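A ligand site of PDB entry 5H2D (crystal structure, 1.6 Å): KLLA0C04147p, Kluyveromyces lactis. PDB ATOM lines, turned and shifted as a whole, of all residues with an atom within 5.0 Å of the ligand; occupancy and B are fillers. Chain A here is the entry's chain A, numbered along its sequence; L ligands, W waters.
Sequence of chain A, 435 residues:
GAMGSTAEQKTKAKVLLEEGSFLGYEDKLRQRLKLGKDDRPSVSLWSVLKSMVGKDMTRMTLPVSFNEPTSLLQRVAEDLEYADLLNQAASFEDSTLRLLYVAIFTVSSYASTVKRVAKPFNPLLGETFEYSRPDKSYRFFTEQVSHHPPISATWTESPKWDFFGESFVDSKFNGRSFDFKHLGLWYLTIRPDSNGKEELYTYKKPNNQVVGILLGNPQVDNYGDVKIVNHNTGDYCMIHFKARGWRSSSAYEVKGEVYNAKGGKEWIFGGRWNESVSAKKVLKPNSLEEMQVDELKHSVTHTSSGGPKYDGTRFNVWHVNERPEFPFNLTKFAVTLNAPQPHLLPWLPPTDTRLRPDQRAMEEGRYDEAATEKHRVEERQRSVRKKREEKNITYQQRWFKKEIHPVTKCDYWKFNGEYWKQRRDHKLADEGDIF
OD1 of Asp 79 lies within hydrogen-bond range of O1 of the ligand (3.0 Å). NZ of Lys 205 sits at hydrogen-bond distance from O1 of the ligand (2.8 Å).
Residues that only touch the ligand: Met 57 (3.6 Å), Leu 62 (3.8 Å), Leu 72 (3.7 Å), Arg 75 (3.7 Å), Tyr 110 (3.7 Å), Arg 116 (3.8 Å), Val 117 (3.7 Å), Ala 118 (3.6 Å), Lys 119 (3.9 Å), Phe 178 (3.6 Å), Phe 180 (3.4 Å), His 182 (3.5 Å), Asn 208 (3.7 Å), Val 210 (3.7 Å) and Val 220 (3.9 Å). Hydrophobic or aromatic side chains within 4 Å of the ligand: Met 57, Leu 62, Leu 72, Tyr 110, Val 117, Phe 178, Phe 180, His 182, Val 210 and Val 220. 17 residues have an atom within 4 Å of the ligand: Met 57, Leu 62, Leu 72, Arg 75, Asp 79, Tyr 110, Arg 116, Val 117, Ala 118, Lys 119, Phe 178, Phe 180, His 182, Lys 205, Asn 208, Val 210 and Val 220. The nearest printed residue that does not touch the ligand is Pro 120 (4.01 Å).
Water W2 lies within hydrogen-bond range of OD1 of Asp 79 (2.7 Å), O of Arg 75 (2.7 Å) and O1 of the ligand (2.8 Å). Water W1 lies within hydrogen-bond range of OH of Tyr 110 (2.8 Å), OD1 of Asp 79 (2.9 Å) and O1 of the ligand (3.3 Å).
The backbone carbonyl oxygen (O) of Asn 208 is in hydrogen-bond range of the backbone NH (N) of Phe 180, 2.8 Å away. The backbone NH of Lys 119 lies within hydrogen-bond range of the backbone carbonyl oxygen of Phe 66. The backbone NH of Val 210 lies within hydrogen-bond range of the backbone carbonyl oxygen of Phe 178, 2.7 Å away. The backbone carbonyl oxygen of Met 57 sits at hydrogen-bond distance from the side-chain amino group of Lys 119 (3.2 Å). The backbone carbonyl oxygen (O) of Tyr 110 is in hydrogen-bond range of the side-chain hydroxyl (OG1) of Thr 113 (2.7 Å). OD2 of Asp 79 is in salt-bridge range of NZ of Lys 205, 2.7 Å away. The side-chain amide oxygen of Asn 208 is in hydrogen-bond range of a ring nitrogen (NE2) of His 182.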
ATOM      1  N   LEU A  45      27.867  24.879   7.960  1.00  0.00           N
ATOM      2  CA  LEU A  45      27.346  24.235   9.164  1.00  0.00           C
ATOM      3  C   LEU A  45      27.826  22.794   9.281  1.00  0.00           C
ATOM      4  O   LEU A  45      28.195  22.341  10.379  1.00  0.00           O
ATOM      5  CB  LEU A  45      25.807  24.287   9.175  1.00  0.00           C
ATOM      6  CG  LEU A  45      25.138  23.744  10.448  1.00  0.00           C
ATOM      7  CD1 LEU A  45      25.721  24.403  11.681  1.00  0.00           C
ATOM      8  CD2 LEU A  45      23.610  23.957  10.390  1.00  0.00           C
ATOM      9  N   LEU A  49      29.493  20.796  12.448  1.00  0.00           N
ATOM     10  CA  LEU A  49      28.760  19.749  13.156  1.00  0.00           C
ATOM     11  C   LEU A  49      29.298  18.346  12.896  1.00  0.00           C
ATOM     12  O   LEU A  49      28.969  17.445  13.657  1.00  0.00           O
ATOM     13  CB  LEU A  49      27.280  19.788  12.794  1.00  0.00           C
ATOM     14  CG  LEU A  49      26.485  21.060  13.146  1.00  0.00           C
ATOM     15  CD1 LEU A  49      25.039  20.917  12.727  1.00  0.00           C
ATOM     16  CD2 LEU A  49      26.589  21.358  14.642  1.00  0.00           C
ATOM     17  N   MET A  57      22.285  20.670  21.617  1.00  0.00           N
ATOM     18  CA  MET A  57      22.587  22.069  21.334  1.00  0.00           C
ATOM     19  C   MET A  57      23.445  22.693  22.436  1.00  0.00           C
ATOM     20  O   MET A  57      24.343  23.501  22.156  1.00  0.00           O
ATOM     21  CB  MET A  57      21.291  22.848  21.164  1.00  0.00           C
ATOM     22  CG  MET A  57      21.373  24.329  21.419  1.00  0.00           C
ATOM     23  SD  MET A  57      19.775  25.080  21.030  1.00  0.00           S
ATOM     24  CE  MET A  57      18.828  24.751  22.530  1.00  0.00           C
ATOM     25  N   LEU A  62      30.090  26.376  19.288  1.00  0.00           N
ATOM     26  CA  LEU A  62      29.822  26.806  17.932  1.00  0.00           C
ATOM     27  C   LEU A  62      30.519  28.133  17.659  1.00  0.00           C
ATOM     28  O   LEU A  62      30.675  28.959  18.563  1.00  0.00           O
ATOM     29  CB  LEU A  62      28.318  26.952  17.683  1.00  0.00           C
ATOM     30  CG  LEU A  62      27.523  25.671  17.926  1.00  0.00           C
ATOM     31  CD1 LEU A  62      26.045  25.983  18.092  1.00  0.00           C
ATOM     32  CD2 LEU A  62      27.720  24.689  16.779  1.00  0.00           C
ATOM     33  N   PHE A  66      27.066  30.830  14.079  1.00  0.00           N
ATOM     34  CA  PHE A  66      25.891  30.007  14.389  1.00  0.00           C
ATOM     35  C   PHE A  66      25.359  30.309  15.781  1.00  0.00           C
ATOM     36  O   PHE A  66      24.676  29.469  16.385  1.00  0.00           O
ATOM     37  CB  PHE A  66      26.217  28.519  14.198  1.00  0.00           C
ATOM     38  CG  PHE A  66      26.440  28.158  12.768  1.00  0.00           C
ATOM     39  CD1 PHE A  66      25.405  28.266  11.855  1.00  0.00           C
ATOM     40  CD2 PHE A  66      27.697  27.792  12.317  1.00  0.00           C
ATOM     41  CE1 PHE A  66      25.602  27.983  10.512  1.00  0.00           C
ATOM     42  CE2 PHE A  66      27.903  27.509  10.977  1.00  0.00           C
ATOM     43  CZ  PHE A  66      26.854  27.604  10.080  1.00  0.00           C
ATOM     44  N   LEU A  72      17.137  32.172  24.800  1.00  0.00           N
ATOM     45  CA  LEU A  72      15.967  31.291  24.749  1.00  0.00           C
ATOM     46  C   LEU A  72      14.754  31.938  25.416  1.00  0.00           C
ATOM     47  O   LEU A  72      13.611  31.784  24.950  1.00  0.00           O
ATOM     48  CB  LEU A  72      16.292  29.939  25.390  1.00  0.00           C
ATOM     49  CG  LEU A  72      16.012  28.681  24.561  1.00  0.00           C
ATOM     50  CD1 LEU A  72      14.540  28.530  24.280  1.00  0.00           C
ATOM     51  CD2 LEU A  72      16.815  28.702  23.262  1.00  0.00           C
ATOM     52  N   ARG A  75      13.314  34.140  22.723  1.00  0.00           N
ATOM     53  CA  ARG A  75      12.672  33.388  21.649  1.00  0.00           C
ATOM     54  C   ARG A  75      11.289  32.912  22.056  1.00  0.00           C
ATOM     55  O   ARG A  75      10.369  32.886  21.239  1.00  0.00           O
ATOM     56  CB  ARG A  75      13.531  32.179  21.240  1.00  0.00           C
ATOM     57  CG  ARG A  75      14.860  32.544  20.626  1.00  0.00           C
ATOM     58  CD  ARG A  75      14.730  33.500  19.440  1.00  0.00           C
ATOM     59  NE  ARG A  75      14.060  32.886  18.295  1.00  0.00           N
ATOM     60  CZ  ARG A  75      14.683  32.240  17.317  1.00  0.00           C
ATOM     61  NH1 ARG A  75      16.016  32.141  17.308  1.00  0.00           N
ATOM     62  NH2 ARG A  75      13.977  31.705  16.329  1.00  0.00           N
ATOM     63  N   VAL A  76      11.122  32.519  23.325  1.00  0.00           N
ATOM     64  CA  VAL A  76       9.805  32.102  23.788  1.00  0.00           C
ATOM     65  C   VAL A  76       8.842  33.287  23.813  1.00  0.00           C
ATOM     66  O   VAL A  76       7.649  33.116  23.540  1.00  0.00           O
ATOM     67  CB  VAL A  76       9.932  31.426  25.168  1.00  0.00           C
ATOM     68  CG1 VAL A  76       8.553  31.181  25.754  1.00  0.00           C
ATOM     69  CG2 VAL A  76      10.711  30.107  25.036  1.00  0.00           C
ATOM     70  N   ASP A  79       6.440  34.028  20.898  1.00  0.00           N
ATOM     71  CA  ASP A  79       5.079  33.496  20.844  1.00  0.00           C
ATOM     72  C   ASP A  79       4.052  34.611  20.738  1.00  0.00           C
ATOM     73  O   ASP A  79       2.951  34.407  20.203  1.00  0.00           O
ATOM     74  CB  ASP A  79       4.715  32.694  22.109  1.00  0.00           C
ATOM     75  CG  ASP A  79       5.380  31.350  22.215  1.00  0.00           C
ATOM     76  OD1 ASP A  79       5.941  30.823  21.216  1.00  0.00           O
ATOM     77  OD2 ASP A  79       5.319  30.810  23.345  1.00  0.00           O
ATOM     78  N   TYR A 110       5.669  30.789  14.039  1.00  0.00           N
ATOM     79  CA  TYR A 110       6.722  30.040  13.368  1.00  0.00           C
ATOM     80  C   TYR A 110       7.323  30.761  12.164  1.00  0.00           C
ATOM     81  O   TYR A 110       8.455  30.448  11.782  1.00  0.00           O
ATOM     82  CB  TYR A 110       6.202  28.619  12.996  1.00  0.00           C
ATOM     83  CG  TYR A 110       6.119  27.904  14.316  1.00  0.00           C
ATOM     84  CD1 TYR A 110       7.276  27.418  14.917  1.00  0.00           C
ATOM     85  CD2 TYR A 110       4.933  27.881  15.034  1.00  0.00           C
ATOM     86  CE1 TYR A 110       7.244  26.876  16.170  1.00  0.00           C
ATOM     87  CE2 TYR A 110       4.899  27.338  16.296  1.00  0.00           C
ATOM     88  CZ  TYR A 110       6.055  26.835  16.864  1.00  0.00           C
ATOM     89  OH  TYR A 110       6.031  26.323  18.123  1.00  0.00           O
ATOM     90  N   THR A 113      10.876  32.007  12.732  1.00  0.00           N
ATOM     91  CA  THR A 113      12.003  31.079  12.859  1.00  0.00           C
ATOM     92  C   THR A 113      12.794  30.938  11.556  1.00  0.00           C
ATOM     93  O   THR A 113      13.955  30.498  11.591  1.00  0.00           O
ATOM     94  CB  THR A 113      11.536  29.686  13.329  1.00  0.00           C
ATOM     95  OG1 THR A 113      10.734  29.044  12.333  1.00  0.00           O
ATOM     96  CG2 THR A 113      10.729  29.787  14.622  1.00  0.00           C
ATOM     97  N   ARG A 116      16.922  32.039  10.545  1.00  0.00           N
ATOM     98  CA  ARG A 116      17.719  32.201  11.756  1.00  0.00           C
ATOM     99  C   ARG A 116      18.261  30.831  12.170  1.00  0.00           C
ATOM    100  O   ARG A 116      17.831  30.231  13.143  1.00  0.00           O
ATOM    101  CB  ARG A 116      16.883  32.866  12.869  1.00  0.00           C
ATOM    102  CG  ARG A 116      16.582  34.335  12.542  1.00  0.00           C
ATOM    103  CD  ARG A 116      15.325  34.771  13.253  1.00  0.00           C
ATOM    104  NE  ARG A 116      15.588  35.010  14.668  1.00  0.00           N
ATOM    105  CZ  ARG A 116      14.664  35.414  15.534  1.00  0.00           C
ATOM    106  NH1 ARG A 116      13.410  35.599  15.117  1.00  0.00           N
ATOM    107  NH2 ARG A 116      15.009  35.626  16.801  1.00  0.00           N
ATOM    108  N   VAL A 117      19.245  30.350  11.403  1.00  0.00           N
ATOM    109  CA  VAL A 117      19.871  29.063  11.683  1.00  0.00           C
ATOM    110  C   VAL A 117      21.018  29.361  12.649  1.00  0.00           C
ATOM    111  O   VAL A 117      22.182  29.546  12.260  1.00  0.00           O
ATOM    112  CB  VAL A 117      20.329  28.358  10.403  1.00  0.00           C
ATOM    113  CG1 VAL A 117      21.008  27.030  10.723  1.00  0.00           C
ATOM    114  CG2 VAL A 117      19.124  28.100   9.489  1.00  0.00           C
ATOM    115  N   ALA A 118      20.692  29.409  13.936  1.00  0.00           N
ATOM    116  CA  ALA A 118      21.625  29.889  14.934  1.00  0.00           C
ATOM    117  C   ALA A 118      21.115  29.537  16.317  1.00  0.00           C
ATOM    118  O   ALA A 118      19.910  29.527  16.563  1.00  0.00           O
ATOM    119  CB  ALA A 118      21.832  31.411  14.832  1.00  0.00           C
ATOM    120  N   LYS A 119      22.067  29.304  17.212  1.00  0.00           N
ATOM    121  CA  LYS A 119      21.766  28.928  18.594  1.00  0.00           C
ATOM    122  C   LYS A 119      21.545  30.186  19.438  1.00  0.00           C
ATOM    123  O   LYS A 119      22.477  30.999  19.573  1.00  0.00           O
ATOM    124  CB  LYS A 119      22.928  28.115  19.152  1.00  0.00           C
ATOM    125  CG  LYS A 119      22.816  27.694  20.608  1.00  0.00           C
ATOM    126  CD  LYS A 119      24.072  26.927  20.999  1.00  0.00           C
ATOM    127  CE  LYS A 119      24.453  27.111  22.448  1.00  0.00           C
ATOM    128  NZ  LYS A 119      25.696  26.340  22.773  1.00  0.00           N
ATOM    129  N   PRO A 120      20.355  30.381  20.018  1.00  0.00           N
ATOM    130  CA  PRO A 120      20.178  31.465  20.996  1.00  0.00           C
ATOM    131  C   PRO A 120      20.974  31.178  22.249  1.00  0.00           C
ATOM    132  O   PRO A 120      21.404  30.051  22.500  1.00  0.00           O
ATOM    133  CB  PRO A 120      18.678  31.446  21.299  1.00  0.00           C
ATOM    134  CG  PRO A 120      18.049  30.598  20.194  1.00  0.00           C
ATOM    135  CD  PRO A 120      19.131  29.580  19.849  1.00  0.00           C
ATOM    136  N   VAL A 169      13.176  22.361  25.813  1.00  0.00           N
ATOM    137  CA  VAL A 169      13.594  22.014  24.467  1.00  0.00           C
ATOM    138  C   VAL A 169      14.627  20.902  24.554  1.00  0.00           C
ATOM    139  O   VAL A 169      15.690  21.075  25.159  1.00  0.00           O
ATOM    140  CB  VAL A 169      14.164  23.236  23.720  1.00  0.00           C
ATOM    141  CG1 VAL A 169      14.588  22.846  22.318  1.00  0.00           C
ATOM    142  CG2 VAL A 169      13.120  24.363  23.673  1.00  0.00           C
ATOM    143  N   PHE A 178      19.194  18.345  12.586  1.00  0.00           N
ATOM    144  CA  PHE A 178      19.198  18.800  13.964  1.00  0.00           C
ATOM    145  C   PHE A 178      17.741  18.922  14.391  1.00  0.00           C
ATOM    146  O   PHE A 178      16.996  19.718  13.825  1.00  0.00           O
ATOM    147  CB  PHE A 178      19.940  20.134  14.100  1.00  0.00           C
ATOM    148  CG  PHE A 178      20.718  20.286  15.388  1.00  0.00           C
ATOM    149  CD1 PHE A 178      20.227  19.814  16.603  1.00  0.00           C
ATOM    150  CD2 PHE A 178      21.945  20.926  15.379  1.00  0.00           C
ATOM    151  CE1 PHE A 178      20.953  19.997  17.767  1.00  0.00           C
ATOM    152  CE2 PHE A 178      22.674  21.110  16.534  1.00  0.00           C
ATOM    153  CZ  PHE A 178      22.186  20.630  17.738  1.00  0.00           C
ATOM    154  N   PHE A 180      14.534  19.272  17.249  1.00  0.00           N
ATOM    155  CA  PHE A 180      14.145  19.989  18.465  1.00  0.00           C
ATOM    156  C   PHE A 180      12.725  19.594  18.842  1.00  0.00           C
ATOM    157  O   PHE A 180      11.799  19.777  18.051  1.00  0.00           O
ATOM    158  CB  PHE A 180      14.254  21.505  18.262  1.00  0.00           C
ATOM    159  CG  PHE A 180      15.631  21.927  17.888  1.00  0.00           C
ATOM    160  CD1 PHE A 180      16.042  21.902  16.553  1.00  0.00           C
ATOM    161  CD2 PHE A 180      16.546  22.267  18.862  1.00  0.00           C
ATOM    162  CE1 PHE A 180      17.358  22.243  16.225  1.00  0.00           C
ATOM    163  CE2 PHE A 180      17.840  22.616  18.539  1.00  0.00           C
ATOM    164  CZ  PHE A 180      18.254  22.599  17.227  1.00  0.00           C
ATOM    165  N   HIS A 182       9.694  20.017  21.881  1.00  0.00           N
ATOM    166  CA  HIS A 182       9.231  20.953  22.909  1.00  0.00           C
ATOM    167  C   HIS A 182       8.314  20.169  23.834  1.00  0.00           C
ATOM    168  O   HIS A 182       7.165  19.868  23.492  1.00  0.00           O
ATOM    169  CB  HIS A 182       8.537  22.138  22.243  1.00  0.00           C
ATOM    170  CG  HIS A 182       9.451  22.890  21.333  1.00  0.00           C
ATOM    171  ND1 HIS A 182       9.991  24.114  21.663  1.00  0.00           N
ATOM    172  CD2 HIS A 182       9.995  22.546  20.136  1.00  0.00           C
ATOM    173  CE1 HIS A 182      10.812  24.501  20.700  1.00  0.00           C
ATOM    174  NE2 HIS A 182      10.836  23.562  19.765  1.00  0.00           N
ATOM    175  N   LYS A 205       3.702  22.449  21.593  1.00  0.00           N
ATOM    176  CA  LYS A 205       4.206  23.063  20.380  1.00  0.00           C
ATOM    177  C   LYS A 205       4.761  22.027  19.414  1.00  0.00           C
ATOM    178  O   LYS A 205       5.175  20.939  19.833  1.00  0.00           O
ATOM    179  CB  LYS A 205       5.279  24.084  20.727  1.00  0.00           C
ATOM    180  CG  LYS A 205       4.740  25.297  21.492  1.00  0.00           C
ATOM    181  CD  LYS A 205       5.875  26.196  21.974  1.00  0.00           C
ATOM    182  CE  LYS A 205       5.336  27.464  22.611  1.00  0.00           C
ATOM    183  NZ  LYS A 205       6.445  28.312  23.163  1.00  0.00           N
ATOM    184  N   ASN A 208      10.738  21.242  15.690  1.00  0.00           N
ATOM    185  CA  ASN A 208      11.493  21.947  14.649  1.00  0.00           C
ATOM    186  C   ASN A 208      12.707  21.113  14.280  1.00  0.00           C
ATOM    187  O   ASN A 208      13.178  20.281  15.061  1.00  0.00           O
ATOM    188  CB  ASN A 208      11.954  23.355  15.087  1.00  0.00           C
ATOM    189  CG  ASN A 208      11.338  23.793  16.383  1.00  0.00           C
ATOM    190  OD1 ASN A 208      11.952  23.646  17.441  1.00  0.00           O
ATOM    191  ND2 ASN A 208      10.118  24.343  16.316  1.00  0.00           N
ATOM    192  N   VAL A 210      16.563  21.468  11.782  1.00  0.00           N
ATOM    193  CA  VAL A 210      17.400  22.075  10.760  1.00  0.00           C
ATOM    194  C   VAL A 210      17.735  20.984   9.771  1.00  0.00           C
ATOM    195  O   VAL A 210      18.314  19.955  10.146  1.00  0.00           O
ATOM    196  CB  VAL A 210      18.672  22.709  11.356  1.00  0.00           C
ATOM    197  CG1 VAL A 210      19.555  23.248  10.254  1.00  0.00           C
ATOM    198  CG2 VAL A 210      18.308  23.829  12.332  1.00  0.00           C
ATOM    199  N   VAL A 220      15.361  26.018   8.418  1.00  0.00           N
ATOM    200  CA  VAL A 220      14.537  25.698   9.577  1.00  0.00           C
ATOM    201  C   VAL A 220      13.183  25.175   9.109  1.00  0.00           C
ATOM    202  O   VAL A 220      12.494  25.830   8.320  1.00  0.00           O
ATOM    203  CB  VAL A 220      14.350  26.931  10.489  1.00  0.00           C
ATOM    204  CG1 VAL A 220      13.491  26.546  11.671  1.00  0.00           C
ATOM    205  CG2 VAL A 220      15.677  27.496  10.934  1.00  0.00           C
HETATM  206  C1  LIG L   1      10.493  27.586  18.274  1.00  0.00           C
HETATM  207  C2  LIG L   1       9.313  28.355  18.873  1.00  0.00           C
HETATM  208  C3  LIG L   1       9.257  28.019  20.335  1.00  0.00           C
HETATM  209  C4  LIG L   1      10.558  28.422  21.023  1.00  0.00           C
HETATM  210  C5  LIG L   1      11.721  27.891  20.368  1.00  0.00           C
HETATM  211  C6  LIG L   1      12.825  27.574  21.135  1.00  0.00           C
HETATM  212  C7  LIG L   1      14.035  27.107  20.565  1.00  0.00           C
HETATM  213  C8  LIG L   1      14.155  26.954  19.178  1.00  0.00           C
HETATM  214  C9  LIG L   1      12.984  27.058  18.385  1.00  0.00           C
HETATM  215  C10 LIG L   1      11.820  27.923  18.949  1.00  0.00           C
HETATM  216  C11 LIG L   1      13.257  27.368  16.852  1.00  0.00           C
HETATM  217  C12 LIG L   1      14.482  26.637  16.311  1.00  0.00           C
HETATM  218  C13 LIG L   1      15.684  26.966  17.224  1.00  0.00           C
HETATM  219  C14 LIG L   1      15.335  26.346  18.591  1.00  0.00           C
HETATM  220  C15 LIG L   1      16.643  26.470  19.336  1.00  0.00           C
HETATM  221  C16 LIG L   1      17.722  26.184  18.255  1.00  0.00           C
HETATM  222  C17 LIG L   1      16.942  26.149  16.920  1.00  0.00           C
HETATM  223  C18 LIG L   1      15.996  28.478  17.272  1.00  0.00           C
HETATM  224  C19 LIG L   1      12.179  29.406  18.672  1.00  0.00           C
HETATM  225  C20 LIG L   1      17.872  26.617  15.768  1.00  0.00           C
HETATM  226  C21 LIG L   1      17.186  26.692  14.410  1.00  0.00           C
HETATM  227  C22 LIG L   1      18.993  25.599  15.703  1.00  0.00           C
HETATM  228  C23 LIG L   1      20.395  25.989  16.051  1.00  0.00           C
HETATM  229  C24 LIG L   1      21.510  24.939  16.011  1.00  0.00           C
HETATM  230  C25 LIG L   1      22.758  25.582  15.383  1.00  0.00           C
HETATM  231  C26 LIG L   1      22.407  26.004  13.952  1.00  0.00           C
HETATM  232  C27 LIG L   1      23.942  24.601  15.309  1.00  0.00           C
HETATM  233  C28 LIG L   1      21.757  24.508  17.446  1.00  0.00           C
HETATM  234  O1  LIG L   1       8.103  28.695  20.970  1.00  0.00           O
HETATM  235  O   HOH W   1       5.266  28.790  19.323  1.00  0.00           O
HETATM  236  O   HOH W   2       8.319  31.420  20.168  1.00  0.00           O
